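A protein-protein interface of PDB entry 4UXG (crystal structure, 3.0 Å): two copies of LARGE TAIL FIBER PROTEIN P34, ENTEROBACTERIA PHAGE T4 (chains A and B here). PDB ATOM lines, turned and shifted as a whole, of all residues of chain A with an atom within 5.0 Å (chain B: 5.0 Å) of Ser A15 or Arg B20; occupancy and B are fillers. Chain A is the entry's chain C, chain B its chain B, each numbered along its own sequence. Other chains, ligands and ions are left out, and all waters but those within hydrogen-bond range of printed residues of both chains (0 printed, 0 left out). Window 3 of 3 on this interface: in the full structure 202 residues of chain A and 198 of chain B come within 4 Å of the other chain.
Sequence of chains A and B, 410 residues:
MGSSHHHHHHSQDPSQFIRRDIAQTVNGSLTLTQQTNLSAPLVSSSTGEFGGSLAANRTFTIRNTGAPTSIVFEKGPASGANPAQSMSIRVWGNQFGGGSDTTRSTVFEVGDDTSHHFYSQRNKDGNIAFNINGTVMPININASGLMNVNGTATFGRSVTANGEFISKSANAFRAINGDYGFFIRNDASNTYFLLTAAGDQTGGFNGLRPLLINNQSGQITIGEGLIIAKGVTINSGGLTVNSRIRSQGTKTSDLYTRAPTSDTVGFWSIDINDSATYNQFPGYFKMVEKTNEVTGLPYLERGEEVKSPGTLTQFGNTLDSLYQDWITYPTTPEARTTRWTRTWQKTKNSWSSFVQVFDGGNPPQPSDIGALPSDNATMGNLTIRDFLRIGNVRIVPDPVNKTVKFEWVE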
ATOM      1  N   ASP A  13     -19.182 -19.280 -20.139  1.00  0.00           N
ATOM      2  CA  ASP A  13     -18.135 -19.675 -21.084  1.00  0.00           C
ATOM      3  C   ASP A  13     -16.867 -18.862 -20.871  1.00  0.00           C
ATOM      4  O   ASP A  13     -16.930 -17.653 -20.648  1.00  0.00           O
ATOM      5  CB  ASP A  13     -18.610 -19.503 -22.534  1.00  0.00           C
ATOM      6  CG  ASP A  13     -19.580 -20.594 -22.978  1.00  0.00           C
ATOM      7  OD1 ASP A  13     -20.139 -21.318 -22.120  1.00  0.00           O
ATOM      8  OD2 ASP A  13     -19.781 -20.723 -24.206  1.00  0.00           O
ATOM      9  N   PRO A  14     -15.703 -19.521 -20.944  1.00  0.00           N
ATOM     10  CA  PRO A  14     -14.441 -18.801 -20.749  1.00  0.00           C
ATOM     11  C   PRO A  14     -14.054 -17.936 -21.943  1.00  0.00           C
ATOM     12  O   PRO A  14     -12.894 -17.562 -22.046  1.00  0.00           O
ATOM     13  CB  PRO A  14     -13.414 -19.928 -20.586  1.00  0.00           C
ATOM     14  CG  PRO A  14     -14.189 -21.143 -20.301  1.00  0.00           C
ATOM     15  CD  PRO A  14     -15.508 -20.976 -20.974  1.00  0.00           C
ATOM     16  N   SER A  15     -15.002 -17.590 -22.801  1.00  0.00           N
ATOM     17  CA  SER A  15     -14.693 -16.778 -23.957  1.00  0.00           C
ATOM     18  C   SER A  15     -15.501 -15.523 -23.797  1.00  0.00           C
ATOM     19  O   SER A  15     -15.552 -14.674 -24.684  1.00  0.00           O
ATOM     20  CB  SER A  15     -15.034 -17.474 -25.273  1.00  0.00           C
ATOM     21  OG  SER A  15     -16.425 -17.436 -25.523  1.00  0.00           O
ATOM     22  N   GLN A  16     -16.163 -15.434 -22.653  1.00  0.00           N
ATOM     23  CA  GLN A  16     -16.899 -14.241 -22.318  1.00  0.00           C
ATOM     24  C   GLN A  16     -16.018 -13.370 -21.445  1.00  0.00           C
ATOM     25  O   GLN A  16     -16.396 -12.262 -21.096  1.00  0.00           O
ATOM     26  CB  GLN A  16     -18.204 -14.577 -21.601  1.00  0.00           C
ATOM     27  CG  GLN A  16     -19.205 -15.326 -22.445  1.00  0.00           C
ATOM     28  CD  GLN A  16     -20.395 -15.793 -21.638  1.00  0.00           C
ATOM     29  OE1 GLN A  16     -20.399 -16.895 -21.098  1.00  0.00           O
ATOM     30  NE2 GLN A  16     -21.406 -14.951 -21.544  1.00  0.00           N
ATOM     31  N   PHE A  17     -14.823 -13.858 -21.132  1.00  0.00           N
ATOM     32  CA  PHE A  17     -13.838 -13.015 -20.493  1.00  0.00           C
ATOM     33  C   PHE A  17     -12.709 -12.716 -21.457  1.00  0.00           C
ATOM     34  O   PHE A  17     -12.427 -13.512 -22.348  1.00  0.00           O
ATOM     35  CB  PHE A  17     -13.290 -13.702 -19.248  1.00  0.00           C
ATOM     36  CG  PHE A  17     -14.333 -14.028 -18.235  1.00  0.00           C
ATOM     37  CD1 PHE A  17     -14.791 -13.067 -17.358  1.00  0.00           C
ATOM     38  CD2 PHE A  17     -14.870 -15.302 -18.167  1.00  0.00           C
ATOM     39  CE1 PHE A  17     -15.765 -13.371 -16.426  1.00  0.00           C
ATOM     40  CE2 PHE A  17     -15.846 -15.611 -17.236  1.00  0.00           C
ATOM     41  CZ  PHE A  17     -16.291 -14.642 -16.366  1.00  0.00           C
ATOM     42  N   ILE A  18     -12.032 -11.591 -21.254  1.00  0.00           N
ATOM     43  CA  ILE A  18     -10.939 -11.225 -22.133  1.00  0.00           C
ATOM     44  C   ILE A  18      -9.745 -12.018 -21.664  1.00  0.00           C
ATOM     45  O   ILE A  18      -9.517 -12.164 -20.464  1.00  0.00           O
ATOM     46  CB  ILE A  18     -10.631  -9.713 -22.111  1.00  0.00           C
ATOM     47  CG1 ILE A  18     -11.881  -8.903 -22.437  1.00  0.00           C
ATOM     48  CG2 ILE A  18      -9.529  -9.374 -23.094  1.00  0.00           C
ATOM     49  CD1 ILE A  18     -11.735  -7.454 -22.128  1.00  0.00           C
ATOM     50  N   GLN A  24      -7.332 -10.275 -28.668  1.00  0.00           N
ATOM     51  CA  GLN A  24      -8.724 -10.391 -28.269  1.00  0.00           C
ATOM     52  C   GLN A  24      -9.545  -9.278 -28.882  1.00  0.00           C
ATOM     53  O   GLN A  24      -9.038  -8.201 -29.147  1.00  0.00           O
ATOM     54  CB  GLN A  24      -8.854 -10.327 -26.751  1.00  0.00           C
ATOM     55  CG  GLN A  24      -8.249 -11.485 -26.033  1.00  0.00           C
ATOM     56  CD  GLN A  24      -9.119 -12.709 -26.089  1.00  0.00           C
ATOM     57  OE1 GLN A  24      -9.990 -12.905 -25.244  1.00  0.00           O
ATOM     58  NE2 GLN A  24      -8.904 -13.536 -27.101  1.00  0.00           N
ATOM     59  N   THR A  25     -10.830  -9.533 -29.056  1.00  0.00           N
ATOM     60  CA  THR A  25     -11.730  -8.538 -29.598  1.00  0.00           C
ATOM     61  C   THR A  25     -12.815  -8.286 -28.564  1.00  0.00           C
ATOM     62  O   THR A  25     -13.570  -9.185 -28.215  1.00  0.00           O
ATOM     63  CB  THR A  25     -12.348  -8.987 -30.916  1.00  0.00           C
ATOM     64  OG1 THR A  25     -11.309  -9.201 -31.881  1.00  0.00           O
ATOM     65  CG2 THR A  25     -13.307  -7.935 -31.425  1.00  0.00           C
ATOM     66  N   VAL A  26     -12.885  -7.059 -28.070  1.00  0.00           N
ATOM     67  CA  VAL A  26     -13.794  -6.723 -26.989  1.00  0.00           C
ATOM     68  C   VAL A  26     -15.088  -6.131 -27.535  1.00  0.00           C
ATOM     69  O   VAL A  26     -15.068  -5.132 -28.258  1.00  0.00           O
ATOM     70  CB  VAL A  26     -13.144  -5.730 -26.023  1.00  0.00           C
ATOM     71  CG1 VAL A  26     -14.069  -5.420 -24.876  1.00  0.00           C
ATOM     72  CG2 VAL A  26     -11.843  -6.286 -25.514  1.00  0.00           C
ATOM     73  N   ASN A  27     -16.213  -6.744 -27.171  1.00  0.00           N
ATOM     74  CA  ASN A  27     -17.512  -6.322 -27.677  1.00  0.00           C
ATOM     75  C   ASN A  27     -18.290  -5.517 -26.650  1.00  0.00           C
ATOM     76  O   ASN A  27     -19.422  -5.122 -26.887  1.00  0.00           O
ATOM     77  CB  ASN A  27     -18.326  -7.541 -28.102  1.00  0.00           C
ATOM     78  CG  ASN A  27     -17.680  -8.314 -29.230  1.00  0.00           C
ATOM     79  OD1 ASN A  27     -17.066  -7.733 -30.119  1.00  0.00           O
ATOM     80  ND2 ASN A  27     -17.773  -9.636 -29.173  1.00  0.00           N
ATOM     81  N   GLY A  28     -17.665  -5.277 -25.506  1.00  0.00           N
ATOM     82  CA  GLY A  28     -18.249  -4.461 -24.465  1.00  0.00           C
ATOM     83  C   GLY A  28     -17.554  -3.130 -24.359  1.00  0.00           C
ATOM     84  O   GLY A  28     -16.426  -2.978 -24.817  1.00  0.00           O
ATOM     85  N   ILE B  18     -12.300  -9.238 -16.225  1.00  0.00           N
ATOM     86  CA  ILE B  18     -12.946  -8.388 -17.209  1.00  0.00           C
ATOM     87  C   ILE B  18     -13.636  -9.258 -18.244  1.00  0.00           C
ATOM     88  O   ILE B  18     -13.062 -10.234 -18.721  1.00  0.00           O
ATOM     89  CB  ILE B  18     -11.957  -7.443 -17.924  1.00  0.00           C
ATOM     90  CG1 ILE B  18     -11.201  -6.587 -16.920  1.00  0.00           C
ATOM     91  CG2 ILE B  18     -12.684  -6.539 -18.892  1.00  0.00           C
ATOM     92  CD1 ILE B  18     -10.045  -5.861 -17.511  1.00  0.00           C
ATOM     93  N   ARG B  19     -14.841  -8.860 -18.631  1.00  0.00           N
ATOM     94  CA  ARG B  19     -15.627  -9.608 -19.592  1.00  0.00           C
ATOM     95  C   ARG B  19     -15.529  -9.019 -20.978  1.00  0.00           C
ATOM     96  O   ARG B  19     -15.315  -7.824 -21.158  1.00  0.00           O
ATOM     97  CB  ARG B  19     -17.086  -9.704 -19.151  1.00  0.00           C
ATOM     98  CG  ARG B  19     -17.246 -10.606 -17.937  1.00  0.00           C
ATOM     99  CD  ARG B  19     -18.685 -10.799 -17.544  1.00  0.00           C
ATOM    100  NE  ARG B  19     -19.464 -11.238 -18.689  1.00  0.00           N
ATOM    101  CZ  ARG B  19     -20.720 -11.650 -18.622  1.00  0.00           C
ATOM    102  NH1 ARG B  19     -21.336 -11.702 -17.451  1.00  0.00           N
ATOM    103  NH2 ARG B  19     -21.351 -12.018 -19.725  1.00  0.00           N
ATOM    104  N   ARG B  20     -15.674  -9.888 -21.962  1.00  0.00           N
ATOM    105  CA  ARG B  20     -15.448  -9.542 -23.349  1.00  0.00           C
ATOM    106  C   ARG B  20     -16.742  -9.261 -24.113  1.00  0.00           C
ATOM    107  O   ARG B  20     -16.708  -8.852 -25.271  1.00  0.00           O
ATOM    108  CB  ARG B  20     -14.673 -10.692 -23.993  1.00  0.00           C
ATOM    109  CG  ARG B  20     -14.137 -10.450 -25.367  1.00  0.00           C
ATOM    110  CD  ARG B  20     -13.586 -11.735 -25.928  1.00  0.00           C
ATOM    111  NE  ARG B  20     -14.671 -12.646 -26.263  1.00  0.00           N
ATOM    112  CZ  ARG B  20     -15.358 -12.626 -27.396  1.00  0.00           C
ATOM    113  NH1 ARG B  20     -15.095 -11.717 -28.329  1.00  0.00           N
ATOM    114  NH2 ARG B  20     -16.327 -13.513 -27.587  1.00  0.00           N
ATOM    115  N   ASP B  21     -17.884  -9.403 -23.446  1.00  0.00           N
ATOM    116  CA  ASP B  21     -19.161  -9.343 -24.151  1.00  0.00           C
ATOM    117  C   ASP B  21     -20.067  -8.202 -23.714  1.00  0.00           C
ATOM    118  O   ASP B  21     -20.954  -7.795 -24.460  1.00  0.00           O
ATOM    119  CB  ASP B  21     -19.933 -10.654 -23.981  1.00  0.00           C
ATOM    120  CG  ASP B  21     -20.039 -11.096 -22.530  1.00  0.00           C
ATOM    121  OD1 ASP B  21     -19.889 -10.255 -21.624  1.00  0.00           O
ATOM    122  OD2 ASP B  21     -20.338 -12.282 -22.292  1.00  0.00           O
ATOM    123  N   ILE B  22     -19.870  -7.707 -22.498  1.00  0.00           N
ATOM    124  CA  ILE B  22     -20.740  -6.668 -21.973  1.00  0.00           C
ATOM    125  C   ILE B  22     -19.935  -5.501 -21.431  1.00  0.00           C
ATOM    126  O   ILE B  22     -18.736  -5.617 -21.198  1.00  0.00           O
ATOM    127  CB  ILE B  22     -21.652  -7.212 -20.854  1.00  0.00           C
ATOM    128  CG1 ILE B  22     -20.817  -7.767 -19.705  1.00  0.00           C
ATOM    129  CG2 ILE B  22     -22.545  -8.298 -21.377  1.00  0.00           C
ATOM    130  CD1 ILE B  22     -21.620  -8.073 -18.488  1.00  0.00           C
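Ile B18 touches Phe A17. Arg B19 touches Phe A17 (CG to CE1, 3.5 Å). Arg B20 touches Phe A17. Arg B19 touches Ile A18 (O to CD1, 3.7 Å). Arg B20 touches Ile A18. Arg B20 touches Gln A24 (CD to OE1, 3.8 Å). Val A26 touches Arg B20. Asp B21 touches Asn A27. Arg B20 touches Gly A28 (O to N, 3.7 Å). Gly A28 touches Ile B22.
O of Ser A15 is in hydrogen-bond range of NE of Arg B20 (2.7 Å). The backbone NH (N) of Arg B20 lies within hydrogen-bond range of the backbone carbonyl oxygen (O) of Gln A16, at 2.6 Å. NH1 of Arg B20 lies within hydrogen-bond range of O of Thr A25 (3.0 Å). The backbone carbonyl oxygen (O) of Arg B20 lies within hydrogen-bond range of the backbone NH (N) of Asn A27 (2.9 Å). The backbone carbonyl oxygen (O) of Ile B18 sits at hydrogen-bond distance from the backbone NH (N) of Ile A18, at 3.1 Å. NH2 of Arg B19 sits close to NE2 of Gln A16 (3.5 Å). The side-chain carboxylate of Asp B21 is in hydrogen-bond range of the side-chain amide nitrogen of Gln A16, at 3.0 Å.
Hydrophobic or aromatic side chains of chain B that line the printed part of chain A: Ile B18. Of the 11 printed residues of chain A, 9 touch a printed residue of chain B. Among the printed residues, no Asp or Glu carboxylate lies within 4 Å of a Lys or Arg side-chain nitrogen of the other chain.
Ile A18 touches its own counterpart, Ile B18. Position printed for both chains: 18.
Asp A13 touches none of the printed residues of chain B. Pro A14 touches none of the printed residues of chain B. Of chain B, only Arg B20 (2.7 Å) comes within 4 Å of Ser A15. Printed residues of chain B within 4 Å of Gln A16: Arg B19 (3.1 Å), Arg B20 (2.6 Å) and Asp B21 (3.0 Å). Of the printed residues of chain B, Val A26 touches Arg B20. Arg B20 touches just these residues of chain A: Ser A15 (2.7 Å), Gln A16 (2.6 Å), Phe A17 (3.8 Å), Ile A18 (3.7 Å), Gln A24 (3.8 Å), Thr A25 (3.0 Å), Val A26 (3.9 Å), Asn A27 (2.9 Å) and Gly A28 (3.7 Å). The nearest printed residue of chain B that does not touch Ser A15 is Asp B21 (5.9 Å). The nearest printed residue of chain A that does not touch Arg B20 is Pro A14 (6.7 Å). The nearest printed residue of chain B that does not touch Asn A27 is Ile B22 (5.0 Å).
OD2 of Asp B21 is in salt-bridge range of NH2 of Arg B19 (2.8 Å). The backbone NH (N) of Asp A13 is in hydrogen-bond range of the side-chain amide oxygen (OE1) of Gln A16 (2.8 Å).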
